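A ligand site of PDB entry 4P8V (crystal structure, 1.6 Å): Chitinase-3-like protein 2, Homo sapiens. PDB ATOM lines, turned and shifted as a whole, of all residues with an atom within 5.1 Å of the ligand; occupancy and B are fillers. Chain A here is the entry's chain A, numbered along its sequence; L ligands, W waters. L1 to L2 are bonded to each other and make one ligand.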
ATOM      1  N   TYR A  13     -21.676  22.332 -16.281  1.00  0.00           N
ATOM      2  CA  TYR A  13     -20.472  21.528 -16.319  1.00  0.00           C
ATOM      3  C   TYR A  13     -19.981  21.233 -14.914  1.00  0.00           C
ATOM      4  O   TYR A  13     -20.040  22.091 -14.012  1.00  0.00           O
ATOM      5  CB  TYR A  13     -19.343  22.227 -17.071  1.00  0.00           C
ATOM      6  CG  TYR A  13     -19.446  22.292 -18.561  1.00  0.00           C
ATOM      7  CD1 TYR A  13     -20.003  23.413 -19.156  1.00  0.00           C
ATOM      8  CD2 TYR A  13     -18.944  21.295 -19.383  1.00  0.00           C
ATOM      9  CE1 TYR A  13     -20.075  23.521 -20.528  1.00  0.00           C
ATOM     10  CE2 TYR A  13     -19.016  21.402 -20.756  1.00  0.00           C
ATOM     11  CZ  TYR A  13     -19.566  22.524 -21.339  1.00  0.00           C
ATOM     12  OH  TYR A  13     -19.612  22.657 -22.721  1.00  0.00           O
ATOM     13  N   TRP A  17     -11.517  16.695 -11.817  1.00  0.00           N
ATOM     14  CA  TRP A  17     -10.315  17.004 -11.019  1.00  0.00           C
ATOM     15  C   TRP A  17     -10.655  17.690  -9.701  1.00  0.00           C
ATOM     16  O   TRP A  17      -9.784  17.829  -8.805  1.00  0.00           O
ATOM     17  CB  TRP A  17      -9.301  17.787 -11.826  1.00  0.00           C
ATOM     18  CG  TRP A  17      -9.803  19.065 -12.378  1.00  0.00           C
ATOM     19  CD1 TRP A  17      -9.797  20.269 -11.763  1.00  0.00           C
ATOM     20  CD2 TRP A  17     -10.365  19.281 -13.683  1.00  0.00           C
ATOM     21  NE1 TRP A  17     -10.357  21.214 -12.571  1.00  0.00           N
ATOM     22  CE2 TRP A  17     -10.727  20.637 -13.756  1.00  0.00           C
ATOM     23  CE3 TRP A  17     -10.650  18.445 -14.779  1.00  0.00           C
ATOM     24  CZ2 TRP A  17     -11.335  21.199 -14.894  1.00  0.00           C
ATOM     25  CZ3 TRP A  17     -11.261  18.986 -15.888  1.00  0.00           C
ATOM     26  CH2 TRP A  17     -11.593  20.361 -15.948  1.00  0.00           C
ATOM     27  N   ARG A  21      -9.356  18.070  -4.596  1.00  0.00           N
ATOM     28  CA  ARG A  21      -9.166  19.287  -3.812  1.00  0.00           C
ATOM     29  C   ARG A  21      -9.556  19.020  -2.379  1.00  0.00           C
ATOM     30  O   ARG A  21     -10.359  18.134  -2.077  1.00  0.00           O
ATOM     31  CB  ARG A  21     -10.009  20.442  -4.387  1.00  0.00           C
ATOM     32  CG  ARG A  21      -9.480  20.958  -5.696  1.00  0.00           C
ATOM     33  CD  ARG A  21     -10.440  21.903  -6.389  1.00  0.00           C
ATOM     34  NE  ARG A  21      -9.820  22.376  -7.615  1.00  0.00           N
ATOM     35  CZ  ARG A  21     -10.489  22.803  -8.687  1.00  0.00           C
ATOM     36  NH1 ARG A  21     -11.801  22.836  -8.708  1.00  0.00           N
ATOM     37  NH2 ARG A  21      -9.810  23.172  -9.740  1.00  0.00           N
ATOM     38  N   PHE A  44     -13.602  15.716 -18.213  1.00  0.00           N
ATOM     39  CA  PHE A  44     -13.751  15.441 -19.634  1.00  0.00           C
ATOM     40  C   PHE A  44     -13.380  13.973 -19.895  1.00  0.00           C
ATOM     41  O   PHE A  44     -12.588  13.357 -19.143  1.00  0.00           O
ATOM     42  CB  PHE A  44     -12.779  16.290 -20.439  1.00  0.00           C
ATOM     43  CG  PHE A  44     -13.032  17.762 -20.389  1.00  0.00           C
ATOM     44  CD1 PHE A  44     -14.037  18.321 -21.174  1.00  0.00           C
ATOM     45  CD2 PHE A  44     -12.250  18.607 -19.633  1.00  0.00           C
ATOM     46  CE1 PHE A  44     -14.254  19.691 -21.162  1.00  0.00           C
ATOM     47  CE2 PHE A  44     -12.456  19.964 -19.626  1.00  0.00           C
ATOM     48  CZ  PHE A  44     -13.461  20.509 -20.393  1.00  0.00           C
ATOM     49  N   GLY A  83     -12.727  17.358 -24.740  1.00  0.00           N
ATOM     50  CA  GLY A  83     -12.009  18.575 -25.040  1.00  0.00           C
ATOM     51  C   GLY A  83     -11.487  19.301 -23.827  1.00  0.00           C
ATOM     52  O   GLY A  83     -10.910  18.695 -22.923  1.00  0.00           O
ATOM     53  N   GLY A  84     -11.662  20.605 -23.817  1.00  0.00           N
ATOM     54  CA  GLY A  84     -11.115  21.453 -22.771  1.00  0.00           C
ATOM     55  C   GLY A  84      -9.773  22.002 -23.106  1.00  0.00           C
ATOM     56  O   GLY A  84      -9.110  21.565 -24.096  1.00  0.00           O
ATOM     57  N   TYR A  85      -9.348  22.972 -22.314  1.00  0.00           N
ATOM     58  CA  TYR A  85      -8.138  23.711 -22.596  1.00  0.00           C
ATOM     59  C   TYR A  85      -6.903  22.810 -22.660  1.00  0.00           C
ATOM     60  O   TYR A  85      -6.099  22.928 -23.598  1.00  0.00           O
ATOM     61  CB  TYR A  85      -7.896  24.790 -21.540  1.00  0.00           C
ATOM     62  CG  TYR A  85      -6.601  25.514 -21.707  1.00  0.00           C
ATOM     63  CD1 TYR A  85      -6.433  26.482 -22.687  1.00  0.00           C
ATOM     64  CD2 TYR A  85      -5.522  25.237 -20.878  1.00  0.00           C
ATOM     65  CE1 TYR A  85      -5.225  27.144 -22.853  1.00  0.00           C
ATOM     66  CE2 TYR A  85      -4.315  25.900 -21.027  1.00  0.00           C
ATOM     67  CZ  TYR A  85      -4.176  26.849 -22.021  1.00  0.00           C
ATOM     68  OH  TYR A  85      -2.976  27.497 -22.165  1.00  0.00           O
ATOM     69  N   LEU A  86      -6.717  21.962 -21.655  1.00  0.00           N
ATOM     70  CA  LEU A  86      -5.497  21.126 -21.575  1.00  0.00           C
ATOM     71  C   LEU A  86      -5.390  20.113 -22.722  1.00  0.00           C
ATOM     72  O   LEU A  86      -4.315  19.880 -23.284  1.00  0.00           O
ATOM     73  CB  LEU A  86      -5.416  20.384 -20.237  1.00  0.00           C
ATOM     74  CG  LEU A  86      -5.058  21.217 -19.002  1.00  0.00           C
ATOM     75  CD1 LEU A  86      -4.983  20.308 -17.785  1.00  0.00           C
ATOM     76  CD2 LEU A  86      -3.722  21.925 -19.200  1.00  0.00           C
ATOM     77  N   PHE A  87      -6.523  19.550 -23.089  1.00  0.00           N
ATOM     78  CA  PHE A  87      -6.603  18.563 -24.169  1.00  0.00           C
ATOM     79  C   PHE A  87      -6.223  19.238 -25.479  1.00  0.00           C
ATOM     80  O   PHE A  87      -5.507  18.682 -26.307  1.00  0.00           O
ATOM     81  CB  PHE A  87      -8.052  18.071 -24.230  1.00  0.00           C
ATOM     82  CG  PHE A  87      -8.269  16.835 -25.063  1.00  0.00           C
ATOM     83  CD1 PHE A  87      -7.889  15.596 -24.607  1.00  0.00           C
ATOM     84  CD2 PHE A  87      -8.932  16.918 -26.270  1.00  0.00           C
ATOM     85  CE1 PHE A  87      -8.129  14.452 -25.344  1.00  0.00           C
ATOM     86  CE2 PHE A  87      -9.204  15.791 -26.998  1.00  0.00           C
ATOM     87  CZ  PHE A  87      -8.802  14.547 -26.547  1.00  0.00           C
ATOM     88  N   ASP A 122     -20.901  16.440 -25.643  1.00  0.00           N
ATOM     89  CA  ASP A 122     -20.453  17.801 -25.837  1.00  0.00           C
ATOM     90  C   ASP A 122     -19.033  17.779 -26.369  1.00  0.00           C
ATOM     91  O   ASP A 122     -18.157  17.128 -25.796  1.00  0.00           O
ATOM     92  CB  ASP A 122     -20.505  18.540 -24.481  1.00  0.00           C
ATOM     93  CG  ASP A 122     -20.004  19.938 -24.561  1.00  0.00           C
ATOM     94  OD1 ASP A 122     -20.674  20.794 -25.220  1.00  0.00           O
ATOM     95  OD2 ASP A 122     -18.929  20.198 -23.981  1.00  0.00           O
ATOM     96  N   SER A 124     -16.043  20.085 -26.802  1.00  0.00           N
ATOM     97  CA  SER A 124     -15.512  21.395 -26.462  1.00  0.00           C
ATOM     98  C   SER A 124     -14.056  21.516 -26.889  1.00  0.00           C
ATOM     99  O   SER A 124     -13.133  21.445 -26.103  1.00  0.00           O
ATOM    100  CB  SER A 124     -15.681  21.707 -24.978  1.00  0.00           C
ATOM    101  OG  SER A 124     -17.032  21.970 -24.651  1.00  0.00           O
ATOM    102  N   ILE A 126     -10.921  23.326 -27.781  1.00  0.00           N
ATOM    103  CA  ILE A 126     -10.348  24.586 -27.363  1.00  0.00           C
ATOM    104  C   ILE A 126      -8.985  24.833 -27.994  1.00  0.00           C
ATOM    105  O   ILE A 126      -7.963  24.313 -27.521  1.00  0.00           O
ATOM    106  CB  ILE A 126     -10.187  24.629 -25.834  1.00  0.00           C
ATOM    107  CG1 ILE A 126     -11.482  24.171 -25.115  1.00  0.00           C
ATOM    108  CG2 ILE A 126      -9.752  26.021 -25.387  1.00  0.00           C
ATOM    109  CD1 ILE A 126     -12.757  24.982 -25.424  1.00  0.00           C
ATOM    110  N   TYR A 127      -8.901  25.616 -29.055  1.00  0.00           N
ATOM    111  CA  TYR A 127      -9.983  26.020 -29.977  1.00  0.00           C
ATOM    112  C   TYR A 127      -9.485  25.596 -31.349  1.00  0.00           C
ATOM    113  O   TYR A 127      -8.274  25.468 -31.531  1.00  0.00           O
ATOM    114  CB  TYR A 127     -10.167  27.530 -29.940  1.00  0.00           C
ATOM    115  CG  TYR A 127     -10.799  28.055 -28.671  1.00  0.00           C
ATOM    116  CD1 TYR A 127     -10.050  28.778 -27.743  1.00  0.00           C
ATOM    117  CD2 TYR A 127     -12.128  27.806 -28.390  1.00  0.00           C
ATOM    118  CE1 TYR A 127     -10.629  29.265 -26.568  1.00  0.00           C
ATOM    119  CE2 TYR A 127     -12.705  28.280 -27.215  1.00  0.00           C
ATOM    120  CZ  TYR A 127     -11.960  29.022 -26.328  1.00  0.00           C
ATOM    121  OH  TYR A 127     -12.539  29.474 -25.141  1.00  0.00           O
ATOM    122  N   LEU A 191     -18.709  29.897 -24.537  1.00  0.00           N
ATOM    123  CA  LEU A 191     -17.679  30.060 -23.491  1.00  0.00           C
ATOM    124  C   LEU A 191     -17.360  31.540 -23.272  1.00  0.00           C
ATOM    125  O   LEU A 191     -16.261  32.038 -23.514  1.00  0.00           O
ATOM    126  CB  LEU A 191     -16.439  29.239 -23.879  1.00  0.00           C
ATOM    127  CG  LEU A 191     -16.718  27.751 -24.071  1.00  0.00           C
ATOM    128  CD1 LEU A 191     -15.529  27.117 -24.777  1.00  0.00           C
ATOM    129  CD2 LEU A 191     -17.012  27.023 -22.766  1.00  0.00           C
ATOM    130  N   PHE A 193     -16.423  33.841 -21.279  1.00  0.00           N
ATOM    131  CA  PHE A 193     -15.541  34.107 -20.145  1.00  0.00           C
ATOM    132  C   PHE A 193     -14.118  33.957 -20.700  1.00  0.00           C
ATOM    133  O   PHE A 193     -13.950  33.714 -21.901  1.00  0.00           O
ATOM    134  CB  PHE A 193     -15.862  33.224 -18.916  1.00  0.00           C
ATOM    135  CG  PHE A 193     -16.291  31.813 -19.242  1.00  0.00           C
ATOM    136  CD1 PHE A 193     -15.364  30.879 -19.664  1.00  0.00           C
ATOM    137  CD2 PHE A 193     -17.595  31.416 -19.085  1.00  0.00           C
ATOM    138  CE1 PHE A 193     -15.757  29.581 -19.930  1.00  0.00           C
ATOM    139  CE2 PHE A 193     -17.988  30.117 -19.369  1.00  0.00           C
ATOM    140  CZ  PHE A 193     -17.051  29.206 -19.790  1.00  0.00           C
ATOM    141  N   ASP A 194     -13.102  34.178 -19.857  1.00  0.00           N
ATOM    142  CA  ASP A 194     -11.693  34.207 -20.264  1.00  0.00           C
ATOM    143  C   ASP A 194     -11.442  35.291 -21.280  1.00  0.00           C
ATOM    144  O   ASP A 194     -10.545  35.208 -22.122  1.00  0.00           O
ATOM    145  CB  ASP A 194     -11.215  32.833 -20.796  1.00  0.00           C
ATOM    146  CG  ASP A 194     -11.267  31.754 -19.742  1.00  0.00           C
ATOM    147  OD1 ASP A 194     -11.040  32.063 -18.535  1.00  0.00           O
ATOM    148  OD2 ASP A 194     -11.499  30.582 -20.142  1.00  0.00           O
ATOM    149  N   TYR A 250     -15.815  31.301 -11.434  1.00  0.00           N
ATOM    150  CA  TYR A 250     -14.460  31.594 -11.007  1.00  0.00           C
ATOM    151  C   TYR A 250     -14.164  33.010 -11.438  1.00  0.00           C
ATOM    152  O   TYR A 250     -14.929  33.593 -12.211  1.00  0.00           O
ATOM    153  CB  TYR A 250     -13.456  30.630 -11.695  1.00  0.00           C
ATOM    154  CG  TYR A 250     -13.392  30.782 -13.202  1.00  0.00           C
ATOM    155  CD1 TYR A 250     -12.418  31.563 -13.786  1.00  0.00           C
ATOM    156  CD2 TYR A 250     -14.342  30.184 -14.048  1.00  0.00           C
ATOM    157  CE1 TYR A 250     -12.345  31.725 -15.160  1.00  0.00           C
ATOM    158  CE2 TYR A 250     -14.265  30.340 -15.399  1.00  0.00           C
ATOM    159  CZ  TYR A 250     -13.301  31.121 -15.960  1.00  0.00           C
ATOM    160  OH  TYR A 250     -13.273  31.284 -17.332  1.00  0.00           O
ATOM    161  N   PHE A 282      -6.342  32.307 -11.183  1.00  0.00           N
ATOM    162  CA  PHE A 282      -7.763  32.151 -10.996  1.00  0.00           C
ATOM    163  C   PHE A 282      -8.096  31.799  -9.564  1.00  0.00           C
ATOM    164  O   PHE A 282      -7.240  31.377  -8.803  1.00  0.00           O
ATOM    165  CB  PHE A 282      -8.394  31.206 -12.064  1.00  0.00           C
ATOM    166  CG  PHE A 282      -8.442  29.730 -11.702  1.00  0.00           C
ATOM    167  CD1 PHE A 282      -7.538  28.848 -12.247  1.00  0.00           C
ATOM    168  CD2 PHE A 282      -9.454  29.233 -10.891  1.00  0.00           C
ATOM    169  CE1 PHE A 282      -7.613  27.481 -11.945  1.00  0.00           C
ATOM    170  CE2 PHE A 282      -9.541  27.872 -10.608  1.00  0.00           C
ATOM    171  CZ  PHE A 282      -8.607  27.008 -11.139  1.00  0.00           C
ATOM    172  N   TRP A 341     -19.817  27.333 -16.045  1.00  0.00           N
ATOM    173  CA  TRP A 341     -18.485  26.763 -15.884  1.00  0.00           C
ATOM    174  C   TRP A 341     -17.871  27.233 -14.553  1.00  0.00           C
ATOM    175  O   TRP A 341     -17.463  28.409 -14.441  1.00  0.00           O
ATOM    176  CB  TRP A 341     -17.530  27.118 -17.010  1.00  0.00           C
ATOM    177  CG  TRP A 341     -16.208  26.405 -16.797  1.00  0.00           C
ATOM    178  CD1 TRP A 341     -15.130  26.847 -16.062  1.00  0.00           C
ATOM    179  CD2 TRP A 341     -15.905  25.047 -17.168  1.00  0.00           C
ATOM    180  NE1 TRP A 341     -14.153  25.864 -16.005  1.00  0.00           N
ATOM    181  CE2 TRP A 341     -14.601  24.765 -16.688  1.00  0.00           C
ATOM    182  CE3 TRP A 341     -16.576  24.067 -17.903  1.00  0.00           C
ATOM    183  CZ2 TRP A 341     -13.989  23.536 -16.893  1.00  0.00           C
ATOM    184  CZ3 TRP A 341     -15.938  22.828 -18.106  1.00  0.00           C
ATOM    185  CH2 TRP A 341     -14.672  22.591 -17.583  1.00  0.00           C
ATOM    186  N   MET A 345     -17.066  24.835  -8.799  1.00  0.00           N
ATOM    187  CA  MET A 345     -16.361  26.036  -8.312  1.00  0.00           C
ATOM    188  C   MET A 345     -17.298  27.058  -7.695  1.00  0.00           C
ATOM    189  O   MET A 345     -16.811  28.038  -7.147  1.00  0.00           O
ATOM    190  CB  MET A 345     -15.522  26.676  -9.397  1.00  0.00           C
ATOM    191  CG  MET A 345     -14.382  25.783  -9.867  1.00  0.00           C
ATOM    192  SD  MET A 345     -13.215  26.602 -10.958  1.00  0.00           S
ATOM    193  CE  MET A 345     -14.276  26.971 -12.336  1.00  0.00           C
HETATM  194  C1  LIG L   1     -12.604  26.548 -21.287  1.00  0.00           C
HETATM  195  C2  LIG L   1     -12.781  25.061 -21.003  1.00  0.00           C
HETATM  196  C3  LIG L   1     -12.038  24.604 -19.758  1.00  0.00           C
HETATM  197  C4  LIG L   1     -11.476  25.778 -18.952  1.00  0.00           C
HETATM  198  C5  LIG L   1     -12.532  26.874 -18.882  1.00  0.00           C
HETATM  199  C6  LIG L   1     -12.120  28.099 -18.041  1.00  0.00           C
HETATM  200  C7  LIG L   1     -14.771  23.848 -21.804  1.00  0.00           C
HETATM  201  C8  LIG L   1     -16.231  23.551 -21.671  1.00  0.00           C
HETATM  202  N1  LIG L   1     -14.192  24.704 -20.936  1.00  0.00           N
HETATM  203  O1  LIG L   1     -11.258  26.819 -21.672  1.00  0.00           O
HETATM  204  O2  LIG L   1     -11.037  23.693 -20.209  1.00  0.00           O
HETATM  205  O3  LIG L   1     -11.268  25.381 -17.607  1.00  0.00           O
HETATM  206  O4  LIG L   1     -12.979  27.319 -20.146  1.00  0.00           O
HETATM  207  O5  LIG L   1     -10.927  28.677 -18.480  1.00  0.00           O
HETATM  208  O6  LIG L   1     -14.108  23.285 -22.682  1.00  0.00           O
HETATM  209  C1  LG2 L   2      -9.962  24.845 -17.327  1.00  0.00           C
HETATM  210  C2  LG2 L   2      -9.768  24.963 -15.826  1.00  0.00           C
HETATM  211  C3  LG2 L   2      -8.440  24.305 -15.381  1.00  0.00           C
HETATM  212  C4  LG2 L   2      -8.335  22.895 -15.952  1.00  0.00           C
HETATM  213  C5  LG2 L   2      -8.611  22.931 -17.460  1.00  0.00           C
HETATM  214  C6  LG2 L   2      -8.621  21.548 -18.080  1.00  0.00           C
HETATM  215  C7  LG2 L   2     -10.868  26.787 -14.644  1.00  0.00           C
HETATM  216  C8  LG2 L   2     -10.776  28.205 -14.192  1.00  0.00           C
HETATM  217  N1  LG2 L   2      -9.850  26.338 -15.341  1.00  0.00           N
HETATM  218  O1  LG2 L   2      -8.391  24.223 -13.965  1.00  0.00           O
HETATM  219  O2  LG2 L   2      -7.049  22.321 -15.713  1.00  0.00           O
HETATM  220  O3  LG2 L   2      -9.905  23.469 -17.681  1.00  0.00           O
HETATM  221  O4  LG2 L   2      -8.798  21.656 -19.489  1.00  0.00           O
HETATM  222  O5  LG2 L   2     -11.876  26.123 -14.381  1.00  0.00           O
HETATM  223  O   HOH W   1      -6.163  23.738 -12.529  1.00  0.00           O
HETATM  224  O   HOH W   2      -8.918  19.440 -21.168  1.00  0.00           O
HETATM  225  O   HOH W   3      -7.468  27.825 -15.967  1.00  0.00           O
HETATM  226  O   HOH W   4      -8.602  27.905 -19.744  1.00  0.00           O
HETATM  227  O   HOH W   5      -7.330  19.894 -14.937  1.00  0.00           O
HETATM  228  O   HOH W   6      -4.727  23.868 -15.731  1.00  0.00           O
HETATM  229  O   HOH W   7     -10.521  24.159 -12.256  1.00  0.00           O
HETATM  230  O   HOH W   8      -9.088  30.054 -16.927  1.00  0.00           O
HETATM  231  O   HOH W   9      -9.139  28.146 -22.530  1.00  0.00           O
HETATM  232  O   HOH W  10     -11.124  29.461 -22.860  1.00  0.00           O
HETATM  233  O   HOH W  11     -13.402  23.878 -13.408  1.00  0.00           O
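Water W7 lies within hydrogen-bond range of an oxygen (O1) of LG2 L2 (2.7 Å), the guanidinium group (NH2) of Arg 21 (2.8 Å) and the indole nitrogen (NE1) of Trp 17 (3.0 Å).
Water W8 lies within hydrogen-bond range of O5 of LIG L1 and OD1 of Asp 194.
Water W2 lies within hydrogen-bond range of O of Gly 83 (2.8 Å), O4 of LG2 L2 (2.8 Å), N of Phe 87 (3.1 Å) and N of Leu 86 (3.4 Å).
Water W11 lies within hydrogen-bond range of an oxygen (O5) of LG2 L2, the indole nitrogen (NE1) of Trp 341 and the side-chain sulfur (SD) of Met 345.
Water W10 lies within hydrogen-bond range of OH of Tyr 127 (2.7 Å), O1 of LIG L1 (2.9 Å) and OD2 of Asp 194 (3.0 Å).
OD2 of Asp 194 sits at hydrogen-bond distance from O5 of LIG L1 (2.6 Å).
N of Tyr 85 is in hydrogen-bond range of O2 of LIG L1 (2.8 Å).
The indole nitrogen (NE1) of Trp 341 sits at hydrogen-bond distance from an oxygen (O5) of LG2 L2 (2.8 Å).
The backbone NH (N) of Leu 86 sits at hydrogen-bond distance from an oxygen (O4) of LG2 L2.
The side-chain sulfur of Met 345 lies close to an oxygen (O5) of LG2 L2 (3.7 Å).
Residues that only touch the ligand: Tyr 13 (3.5 Å), Trp 17 (3.6 Å), Phe 44 (3.7 Å), Gly 84 (3.4 Å), Ser 124 (3.2 Å), Ile 126 (3.5 Å), Leu 191 (3.7 Å), Phe 193 (3.6 Å), Tyr 250 (3.5 Å) and Phe 282 (3.7 Å).
15 residues have an atom within 4 Å of the ligand: Tyr 13, Trp 17, Phe 44, Gly 84, Tyr 85, Leu 86, Ser 124, Ile 126, Leu 191, Phe 193, Asp 194, Tyr 250, Phe 282, Trp 341 and Met 345.
The nearest printed residue that does not touch the ligand is Tyr 127 (4.6 Å).
OD1 of Asp 194 lies within hydrogen-bond range of OH of Tyr 250, at 2.7 Å.
O of Ser 124 sits at hydrogen-bond distance from N of Gly 84, 2.8 Å away.
The side-chain hydroxyl (OG) of Ser 124 is in hydrogen-bond range of the side-chain hydroxyl (OH) of Tyr 13 (3.3 Å).
The side-chain hydroxyl (OG) of Ser 124 is in hydrogen-bond range of the side-chain carboxylate (OD2) of Asp 122 (2.7 Å).
The side-chain hydroxyl of Tyr 13 sits at hydrogen-bond distance from the side-chain carboxylate of Asp 122 (2.8 Å).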
